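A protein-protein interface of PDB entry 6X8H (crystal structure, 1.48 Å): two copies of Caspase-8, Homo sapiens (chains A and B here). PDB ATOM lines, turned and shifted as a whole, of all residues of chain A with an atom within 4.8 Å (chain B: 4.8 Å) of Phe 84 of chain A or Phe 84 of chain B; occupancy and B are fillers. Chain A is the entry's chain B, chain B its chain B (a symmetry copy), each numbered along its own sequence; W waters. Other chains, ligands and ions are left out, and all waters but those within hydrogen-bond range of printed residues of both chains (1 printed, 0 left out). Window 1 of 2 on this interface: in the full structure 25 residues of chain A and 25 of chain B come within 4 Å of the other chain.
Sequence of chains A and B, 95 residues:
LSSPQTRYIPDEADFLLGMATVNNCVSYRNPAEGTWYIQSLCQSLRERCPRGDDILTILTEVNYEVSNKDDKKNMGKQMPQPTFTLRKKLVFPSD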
ATOM      1  N   PHE A  15      19.494  18.507  -2.542  1.00  0.00           N
ATOM      2  CA  PHE A  15      18.317  17.754  -3.002  1.00  0.00           C
ATOM      3  C   PHE A  15      18.329  17.592  -4.512  1.00  0.00           C
ATOM      4  O   PHE A  15      18.791  18.458  -5.269  1.00  0.00           O
ATOM      5  CB  PHE A  15      17.014  18.486  -2.645  1.00  0.00           C
ATOM      6  CG  PHE A  15      16.530  18.261  -1.235  1.00  0.00           C
ATOM      7  CD1 PHE A  15      17.020  19.052  -0.209  1.00  0.00           C
ATOM      8  CD2 PHE A  15      15.548  17.300  -0.957  1.00  0.00           C
ATOM      9  CE1 PHE A  15      16.579  18.864   1.091  1.00  0.00           C
ATOM     10  CE2 PHE A  15      15.094  17.100   0.333  1.00  0.00           C
ATOM     11  CZ  PHE A  15      15.585  17.886   1.387  1.00  0.00           C
ATOM     12  N   LEU A  16      17.762  16.492  -4.931  1.00  0.00           N
ATOM     13  CA  LEU A  16      17.480  16.283  -6.363  1.00  0.00           C
ATOM     14  C   LEU A  16      16.037  15.793  -6.475  1.00  0.00           C
ATOM     15  O   LEU A  16      15.709  14.838  -5.865  1.00  0.00           O
ATOM     16  CB  LEU A  16      18.455  15.271  -6.959  1.00  0.00           C
ATOM     17  CG  LEU A  16      18.115  14.788  -8.364  1.00  0.00           C
ATOM     18  CD1 LEU A  16      18.079  15.921  -9.355  1.00  0.00           C
ATOM     19  CD2 LEU A  16      19.133  13.754  -8.824  1.00  0.00           C
ATOM     20  N   LEU A  56      22.860  14.094 -13.271  1.00  0.00           N
ATOM     21  CA  LEU A  56      22.277  15.147 -14.112  1.00  0.00           C
ATOM     22  C   LEU A  56      22.445  14.812 -15.583  1.00  0.00           C
ATOM     23  O   LEU A  56      21.536  15.041 -16.391  1.00  0.00           O
ATOM     24  CB  LEU A  56      22.919  16.496 -13.800  1.00  0.00           C
ATOM     25  CG  LEU A  56      22.588  16.962 -12.389  1.00  0.00           C
ATOM     26  CD1 LEU A  56      23.094  18.399 -12.169  1.00  0.00           C
ATOM     27  CD2 LEU A  56      21.084  16.796 -12.055  1.00  0.00           C
ATOM     28  N   LEU A  59      19.827  12.113 -16.163  1.00  0.00           N
ATOM     29  CA  LEU A  59      18.474  12.676 -16.261  1.00  0.00           C
ATOM     30  C   LEU A  59      18.270  13.500 -17.526  1.00  0.00           C
ATOM     31  O   LEU A  59      17.141  13.605 -18.011  1.00  0.00           O
ATOM     32  CB  LEU A  59      18.152  13.498 -15.004  1.00  0.00           C
ATOM     33  CG  LEU A  59      17.849  12.662 -13.763  1.00  0.00           C
ATOM     34  CD1 LEU A  59      17.720  13.578 -12.553  1.00  0.00           C
ATOM     35  CD2 LEU A  59      16.586  11.874 -13.930  1.00  0.00           C
ATOM     36  N   THR A  60      19.317  14.117 -18.054  1.00  0.00           N
ATOM     37  CA  THR A  60      19.227  14.737 -19.369  1.00  0.00           C
ATOM     38  C   THR A  60      18.890  13.705 -20.445  1.00  0.00           C
ATOM     39  O   THR A  60      18.063  13.964 -21.330  1.00  0.00           O
ATOM     40  CB  THR A  60      20.543  15.429 -19.710  1.00  0.00           C
ATOM     41  OG1 THR A  60      20.791  16.455 -18.738  1.00  0.00           O
ATOM     42  CG2 THR A  60      20.422  16.132 -21.054  1.00  0.00           C
ATOM     43  N   ASN A  63      15.309  12.873 -20.205  1.00  0.00           N
ATOM     44  CA  ASN A  63      14.537  13.894 -20.899  1.00  0.00           C
ATOM     45  C   ASN A  63      14.539  13.642 -22.407  1.00  0.00           C
ATOM     46  O   ASN A  63      13.492  13.738 -23.061  1.00  0.00           O
ATOM     47  CB  ASN A  63      15.107  15.287 -20.619  1.00  0.00           C
ATOM     48  CG  ASN A  63      14.743  15.809 -19.234  1.00  0.00           C
ATOM     49  OD1 ASN A  63      13.941  15.216 -18.529  1.00  0.00           O
ATOM     50  ND2 ASN A  63      15.316  16.958 -18.864  1.00  0.00           N
ATOM     51  N   PRO A  80       9.659  15.313 -18.873  1.00  0.00           N
ATOM     52  CA  PRO A  80      10.139  15.255 -17.487  1.00  0.00           C
ATOM     53  C   PRO A  80      10.960  16.487 -17.162  1.00  0.00           C
ATOM     54  O   PRO A  80      11.340  17.283 -18.025  1.00  0.00           O
ATOM     55  CB  PRO A  80      10.997  13.984 -17.438  1.00  0.00           C
ATOM     56  CG  PRO A  80      10.553  13.162 -18.653  1.00  0.00           C
ATOM     57  CD  PRO A  80      10.221  14.229 -19.702  1.00  0.00           C
ATOM     58  N   GLN A  81      11.171  16.674 -15.837  1.00  0.00           N
ATOM     59  CA  GLN A  81      11.759  17.910 -15.340  1.00  0.00           C
ATOM     60  C   GLN A  81      12.482  17.725 -14.016  1.00  0.00           C
ATOM     61  O   GLN A  81      11.828  17.729 -12.968  1.00  0.00           O
ATOM     62  CB  GLN A  81      10.651  18.957 -15.194  1.00  0.00           C
ATOM     63  CG  GLN A  81      11.139  20.390 -14.957  1.00  0.00           C
ATOM     64  CD  GLN A  81       9.984  21.300 -14.562  1.00  0.00           C
ATOM     65  OE1 GLN A  81       9.256  21.028 -13.636  1.00  0.00           O
ATOM     66  NE2 GLN A  81       9.794  22.358 -15.326  1.00  0.00           N
ATOM     67  N   PRO A  82      13.810  17.622 -14.014  1.00  0.00           N
ATOM     68  CA  PRO A  82      14.538  17.628 -12.744  1.00  0.00           C
ATOM     69  C   PRO A  82      14.722  19.030 -12.216  1.00  0.00           C
ATOM     70  O   PRO A  82      14.779  20.010 -12.971  1.00  0.00           O
ATOM     71  CB  PRO A  82      15.915  17.050 -13.112  1.00  0.00           C
ATOM     72  CG  PRO A  82      15.728  16.398 -14.433  1.00  0.00           C
ATOM     73  CD  PRO A  82      14.695  17.221 -15.125  1.00  0.00           C
ATOM     74  N   THR A  83      14.789  19.131 -10.885  1.00  0.00           N
ATOM     75  CA  THR A  83      15.135  20.352 -10.182  1.00  0.00           C
ATOM     76  C   THR A  83      16.120  19.970  -9.091  1.00  0.00           C
ATOM     77  O   THR A  83      16.009  18.897  -8.508  1.00  0.00           O
ATOM     78  CB  THR A  83      13.892  20.931  -9.494  1.00  0.00           C
ATOM     79  OG1 THR A  83      12.842  21.154 -10.433  1.00  0.00           O
ATOM     80  CG2 THR A  83      14.224  22.264  -8.890  1.00  0.00           C
ATOM     81  N   PHE A  84      17.092  20.834  -8.807  1.00  0.00           N
ATOM     82  CA  PHE A  84      18.138  20.393  -7.887  1.00  0.00           C
ATOM     83  C   PHE A  84      18.746  21.519  -7.059  1.00  0.00           C
ATOM     84  O   PHE A  84      18.888  22.658  -7.503  1.00  0.00           O
ATOM     85  CB  PHE A  84      19.226  19.568  -8.608  1.00  0.00           C
ATOM     86  CG  PHE A  84      20.075  20.345  -9.601  1.00  0.00           C
ATOM     87  CD1 PHE A  84      19.642  20.494 -10.929  1.00  0.00           C
ATOM     88  CD2 PHE A  84      21.338  20.837  -9.246  1.00  0.00           C
ATOM     89  CE1 PHE A  84      20.425  21.138 -11.868  1.00  0.00           C
ATOM     90  CE2 PHE A  84      22.151  21.490 -10.208  1.00  0.00           C
ATOM     91  CZ  PHE A  84      21.679  21.645 -11.518  1.00  0.00           C
ATOM     92  N   THR A  85      19.115  21.181  -5.819  1.00  0.00           N
ATOM     93  CA  THR A  85      20.006  22.015  -5.015  1.00  0.00           C
ATOM     94  C   THR A  85      21.313  21.286  -4.711  1.00  0.00           C
ATOM     95  O   THR A  85      22.016  21.632  -3.755  1.00  0.00           O
ATOM     96  CB  THR A  85      19.310  22.490  -3.738  1.00  0.00           C
ATOM     97  OG1 THR A  85      18.895  21.333  -3.008  1.00  0.00           O
ATOM     98  CG2 THR A  85      18.070  23.341  -4.058  1.00  0.00           C
ATOM     99  N   LEU A  86      21.658  20.299  -5.525  1.00  0.00           N
ATOM    100  CA  LEU A  86      22.924  19.600  -5.372  1.00  0.00           C
ATOM    101  C   LEU A  86      24.060  20.597  -5.497  1.00  0.00           C
ATOM    102  O   LEU A  86      24.019  21.504  -6.330  1.00  0.00           O
ATOM    103  CB  LEU A  86      23.071  18.559  -6.487  1.00  0.00           C
ATOM    104  CG  LEU A  86      22.045  17.437  -6.530  1.00  0.00           C
ATOM    105  CD1 LEU A  86      22.414  16.541  -7.701  1.00  0.00           C
ATOM    106  CD2 LEU A  86      22.036  16.635  -5.236  1.00  0.00           C
ATOM    107  N   PHE B  15      14.342  23.765 -22.001  1.00  0.00           N
ATOM    108  CA  PHE B  15      14.437  24.952 -21.138  1.00  0.00           C
ATOM    109  C   PHE B  15      15.411  24.719 -19.996  1.00  0.00           C
ATOM    110  O   PHE B  15      15.559  23.608 -19.466  1.00  0.00           O
ATOM    111  CB  PHE B  15      13.080  25.288 -20.502  1.00  0.00           C
ATOM    112  CG  PHE B  15      12.149  26.082 -21.383  1.00  0.00           C
ATOM    113  CD1 PHE B  15      11.335  25.421 -22.288  1.00  0.00           C
ATOM    114  CD2 PHE B  15      12.055  27.475 -21.261  1.00  0.00           C
ATOM    115  CE1 PHE B  15      10.468  26.134 -23.101  1.00  0.00           C
ATOM    116  CE2 PHE B  15      11.194  28.203 -22.059  1.00  0.00           C
ATOM    117  CZ  PHE B  15      10.367  27.552 -22.988  1.00  0.00           C
ATOM    118  N   LEU B  16      16.025  25.799 -19.595  1.00  0.00           N
ATOM    119  CA  LEU B  16      16.825  25.801 -18.356  1.00  0.00           C
ATOM    120  C   LEU B  16      16.417  27.035 -17.553  1.00  0.00           C
ATOM    121  O   LEU B  16      16.479  28.096 -18.063  1.00  0.00           O
ATOM    122  CB  LEU B  16      18.317  25.822 -18.681  1.00  0.00           C
ATOM    123  CG  LEU B  16      19.238  26.072 -17.492  1.00  0.00           C
ATOM    124  CD1 LEU B  16      19.088  25.013 -16.432  1.00  0.00           C
ATOM    125  CD2 LEU B  16      20.688  26.115 -17.954  1.00  0.00           C
ATOM    126  N   LEU B  56      25.035  22.532 -16.521  1.00  0.00           N
ATOM    127  CA  LEU B  56      24.554  21.907 -15.283  1.00  0.00           C
ATOM    128  C   LEU B  56      25.697  21.716 -14.300  1.00  0.00           C
ATOM    129  O   LEU B  56      25.530  21.919 -13.092  1.00  0.00           O
ATOM    130  CB  LEU B  56      23.888  20.568 -15.586  1.00  0.00           C
ATOM    131  CG  LEU B  56      22.612  20.747 -16.396  1.00  0.00           C
ATOM    132  CD1 LEU B  56      21.871  19.405 -16.529  1.00  0.00           C
ATOM    133  CD2 LEU B  56      21.714  21.877 -15.834  1.00  0.00           C
ATOM    134  N   LEU B  59      26.289  25.228 -12.964  1.00  0.00           N
ATOM    135  CA  LEU B  59      25.269  25.617 -11.981  1.00  0.00           C
ATOM    136  C   LEU B  59      25.376  24.833 -10.679  1.00  0.00           C
ATOM    137  O   LEU B  59      24.984  25.339  -9.627  1.00  0.00           O
ATOM    138  CB  LEU B  59      23.866  25.489 -12.595  1.00  0.00           C
ATOM    139  CG  LEU B  59      23.507  26.590 -13.588  1.00  0.00           C
ATOM    140  CD1 LEU B  59      22.178  26.260 -14.253  1.00  0.00           C
ATOM    141  CD2 LEU B  59      23.410  27.924 -12.914  1.00  0.00           C
ATOM    142  N   THR B  60      25.862  23.601 -10.724  1.00  0.00           N
ATOM    143  CA  THR B  60      26.185  22.886  -9.496  1.00  0.00           C
ATOM    144  C   THR B  60      27.259  23.623  -8.695  1.00  0.00           C
ATOM    145  O   THR B  60      27.162  23.735  -7.465  1.00  0.00           O
ATOM    146  CB  THR B  60      26.661  21.475  -9.824  1.00  0.00           C
ATOM    147  OG1 THR B  60      25.602  20.774 -10.494  1.00  0.00           O
ATOM    148  CG2 THR B  60      26.934  20.711  -8.536  1.00  0.00           C
ATOM    149  N   ASN B  63      25.709  26.515  -7.020  1.00  0.00           N
ATOM    150  CA  ASN B  63      25.062  26.064  -5.796  1.00  0.00           C
ATOM    151  C   ASN B  63      26.085  25.905  -4.670  1.00  0.00           C
ATOM    152  O   ASN B  63      25.837  26.329  -3.533  1.00  0.00           O
ATOM    153  CB  ASN B  63      24.347  24.729  -6.021  1.00  0.00           C
ATOM    154  CG  ASN B  63      23.035  24.880  -6.781  1.00  0.00           C
ATOM    155  OD1 ASN B  63      22.564  25.984  -7.011  1.00  0.00           O
ATOM    156  ND2 ASN B  63      22.421  23.748  -7.135  1.00  0.00           N
ATOM    157  N   PRO B  80      20.400  28.475  -4.260  1.00  0.00           N
ATOM    158  CA  PRO B  80      19.897  28.543  -5.638  1.00  0.00           C
ATOM    159  C   PRO B  80      19.392  27.184  -6.081  1.00  0.00           C
ATOM    160  O   PRO B  80      19.600  26.152  -5.438  1.00  0.00           O
ATOM    161  CB  PRO B  80      21.117  28.980  -6.463  1.00  0.00           C
ATOM    162  CG  PRO B  80      22.082  29.592  -5.442  1.00  0.00           C
ATOM    163  CD  PRO B  80      21.847  28.752  -4.182  1.00  0.00           C
ATOM    164  N   GLN B  81      18.630  27.218  -7.200  1.00  0.00           N
ATOM    165  CA  GLN B  81      17.897  26.041  -7.643  1.00  0.00           C
ATOM    166  C   GLN B  81      17.640  26.038  -9.141  1.00  0.00           C
ATOM    167  O   GLN B  81      16.684  26.680  -9.589  1.00  0.00           O
ATOM    168  CB  GLN B  81      16.571  25.972  -6.881  1.00  0.00           C
ATOM    169  CG  GLN B  81      15.812  24.647  -7.016  1.00  0.00           C
ATOM    170  CD  GLN B  81      14.403  24.766  -6.454  1.00  0.00           C
ATOM    171  OE1 GLN B  81      13.648  25.634  -6.827  1.00  0.00           O
ATOM    172  NE2 GLN B  81      14.085  23.912  -5.500  1.00  0.00           N
ATOM    173  N   PRO B  82      18.417  25.296  -9.929  1.00  0.00           N
ATOM    174  CA  PRO B  82      18.075  25.135 -11.344  1.00  0.00           C
ATOM    175  C   PRO B  82      17.005  24.088 -11.540  1.00  0.00           C
ATOM    176  O   PRO B  82      16.864  23.143 -10.754  1.00  0.00           O
ATOM    177  CB  PRO B  82      19.384  24.635 -11.978  1.00  0.00           C
ATOM    178  CG  PRO B  82      20.444  24.936 -10.983  1.00  0.00           C
ATOM    179  CD  PRO B  82      19.778  24.796  -9.656  1.00  0.00           C
ATOM    180  N   THR B  83      16.215  24.279 -12.601  1.00  0.00           N
ATOM    181  CA  THR B  83      15.244  23.309 -13.071  1.00  0.00           C
ATOM    182  C   THR B  83      15.383  23.239 -14.582  1.00  0.00           C
ATOM    183  O   THR B  83      15.651  24.249 -15.223  1.00  0.00           O
ATOM    184  CB  THR B  83      13.823  23.799 -12.765  1.00  0.00           C
ATOM    185  OG1 THR B  83      13.659  24.063 -11.372  1.00  0.00           O
ATOM    186  CG2 THR B  83      12.831  22.731 -13.122  1.00  0.00           C
ATOM    187  N   PHE B  84      15.209  22.054 -15.163  1.00  0.00           N
ATOM    188  CA  PHE B  84      15.515  21.953 -16.588  1.00  0.00           C
ATOM    189  C   PHE B  84      14.672  20.921 -17.329  1.00  0.00           C
ATOM    190  O   PHE B  84      14.301  19.874 -16.799  1.00  0.00           O
ATOM    191  CB  PHE B  84      17.024  21.735 -16.836  1.00  0.00           C
ATOM    192  CG  PHE B  84      17.570  20.398 -16.364  1.00  0.00           C
ATOM    193  CD1 PHE B  84      18.008  20.247 -15.039  1.00  0.00           C
ATOM    194  CD2 PHE B  84      17.742  19.328 -17.255  1.00  0.00           C
ATOM    195  CE1 PHE B  84      18.571  19.062 -14.602  1.00  0.00           C
ATOM    196  CE2 PHE B  84      18.329  18.114 -16.815  1.00  0.00           C
ATOM    197  CZ  PHE B  84      18.732  17.987 -15.480  1.00  0.00           C
ATOM    198  N   THR B  85      14.367  21.233 -18.593  1.00  0.00           N
ATOM    199  CA  THR B  85      13.870  20.241 -19.544  1.00  0.00           C
ATOM    200  C   THR B  85      14.848  20.052 -20.701  1.00  0.00           C
ATOM    201  O   THR B  85      14.464  19.579 -21.776  1.00  0.00           O
ATOM    202  CB  THR B  85      12.470  20.608 -20.038  1.00  0.00           C
ATOM    203  OG1 THR B  85      12.542  21.903 -20.640  1.00  0.00           O
ATOM    204  CG2 THR B  85      11.461  20.659 -18.878  1.00  0.00           C
ATOM    205  N   LEU B  86      16.111  20.394 -20.487  1.00  0.00           N
ATOM    206  CA  LEU B  86      17.135  20.173 -21.495  1.00  0.00           C
ATOM    207  C   LEU B  86      17.203  18.693 -21.819  1.00  0.00           C
ATOM    208  O   LEU B  86      17.098  17.845 -20.932  1.00  0.00           O
ATOM    209  CB  LEU B  86      18.497  20.609 -20.944  1.00  0.00           C
ATOM    210  CG  LEU B  86      18.664  22.076 -20.579  1.00  0.00           C
ATOM    211  CD1 LEU B  86      20.087  22.251 -20.077  1.00  0.00           C
ATOM    212  CD2 LEU B  86      18.410  22.983 -21.775  1.00  0.00           C
HETATM  213  O   HOH W   1      11.117  23.466 -10.106  1.00  0.00           O
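O of Pro 82 of chain A sits at hydrogen-bond distance from N of Phe 84 of chain B (3.0 Å). OG1 of Thr 83 of chain A sits close to OG1 of Thr 83 of chain B, at 3.2 Å. The side-chain amide nitrogen of Asn 63 of chain B is in hydrogen-bond range of the backbone carbonyl oxygen of Leu 86 of chain A (2.9 Å). The backbone carbonyl oxygen (O) of Leu 86 of chain B is in hydrogen-bond range of the side-chain amide nitrogen (ND2) of Asn 63 of chain A, 2.9 Å away. The backbone NH (N) of Phe 84 of chain A lies within hydrogen-bond range of the backbone carbonyl oxygen (O) of Pro 82 of chain B, 3.0 Å away.
Water W1 bridges the side-chain hydroxyl (OG1) of Thr 83 of chain B (2.9 Å) and the side-chain hydroxyl (OG1) of Thr 83 of chain A (2.9 Å).
Of the 13 printed residues of chain A, 10 touch a printed residue of chain B. Hydrophobic or aromatic side chains of chain A within 4 Å of the printed part of chain B: Leu 56, Pro 82 and Phe 84. Of the 13 printed residues of chain B, 10 touch a printed residue of chain A. Printed residues of chain B that touch a printed residue of chain A: Leu 56, Thr 60, Asn 63, Pro 80, Gln 81, Pro 82, Thr 83, Phe 84, Thr 85 and Leu 86.
The backbone carbonyl oxygen (O) of Leu 56 of chain A sits at hydrogen-bond distance from the side-chain hydroxyl (OG1) of Thr 60 of chain A (2.8 Å). The backbone carbonyl oxygen (O) of Phe 15 of chain A sits at hydrogen-bond distance from the backbone NH (N) of Thr 85 of chain A, 2.8 Å away. O of Phe 15 of chain B lies within hydrogen-bond range of N of Leu 86 of chain B. O of Leu 56 of chain B sits at hydrogen-bond distance from OG1 of Thr 60 of chain B, at 2.8 Å. The side-chain amide oxygen (OD1) of Asn 63 of chain A lies close to the backbone carbonyl oxygen (O) of Pro 80 of chain A, at 3.4 Å. OD1 of Asn 63 of chain B sits close to O of Pro 80 of chain B (3.4 Å).
Asn 63 of chain A touches Leu 86 of chain B, and with the chains exchanged Leu 86 of chain A touches Asn 63 of chain B. Pro 82 of chain A touches Thr 83 of chain B, and with the chains exchanged Thr 83 of chain A touches Pro 82 of chain B. Pro 82 of chain A touches Phe 84 of chain B, and with the chains exchanged Phe 84 of chain A touches Pro 82 of chain B. Phe 84 of chain B touches its own counterpart, Phe 84 of chain A.
Of the printed residues of chain B, Leu 56 of chain A touches Thr 60 (3.8 Å). Of the printed residues of chain B, Pro 80 of chain A touches Thr 85. Of the printed residues of chain B, Phe 84 of chain A touches Thr 60 (3.5 Å), Asn 63 (3.7 Å), Gln 81 (3.5 Å), Pro 82 (3.0 Å) and Phe 84 (3.9 Å). Of the printed residues of chain A, Asn 63 of chain B touches Phe 84, Thr 85 and Leu 86. Phe 84 of chain B touches just these residues of chain A: Thr 60, Asn 63, Gln 81, Pro 82 and Phe 84. Of the printed residues of chain A, Thr 85 of chain B touches Asn 63, Pro 80 and Gln 81. The nearest residue of chain B that does not touch Phe 84 of chain A is Pro 80 of chain B (4.1 Å).
Among the printed residues, merely in contact across the chains: Thr 83 of chain A with Pro 82 of chain B, Pro 82 of chain A with Thr 83 of chain B, Gln 81 of chain A with Thr 83 of chain B, Thr 83 of chain A with Gln 81 of chain B, Pro 80 of chain A with Thr 85 of chain B, Thr 85 of chain A with Pro 80 of chain B, Phe 84 of chain A with Gln 81 of chain B, Gln 81 of chain A with Phe 84 of chain B, Phe 84 of chain A with Thr 60 of chain B, Thr 60 of chain A with Phe 84 of chain B, Thr 85 of chain A with Asn 63 of chain B, Asn 63 of chain A with Thr 85 of chain B, Asn 63 of chain A with Phe 84 of chain B, Phe 84 of chain A with Asn 63 of chain B, Leu 86 of chain A with Thr 60 of chain B, Thr 60 of chain A with Leu 86 of chain B, Leu 56 of chain A with Thr 60 of chain B, Thr 60 of chain A with Leu 56 of chain B, Phe 84 of chain A with Phe 84 of chain B, Gln 81 of chain A with Thr 85 of chain B and Thr 85 of chain A with Gln 81 of chain B.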
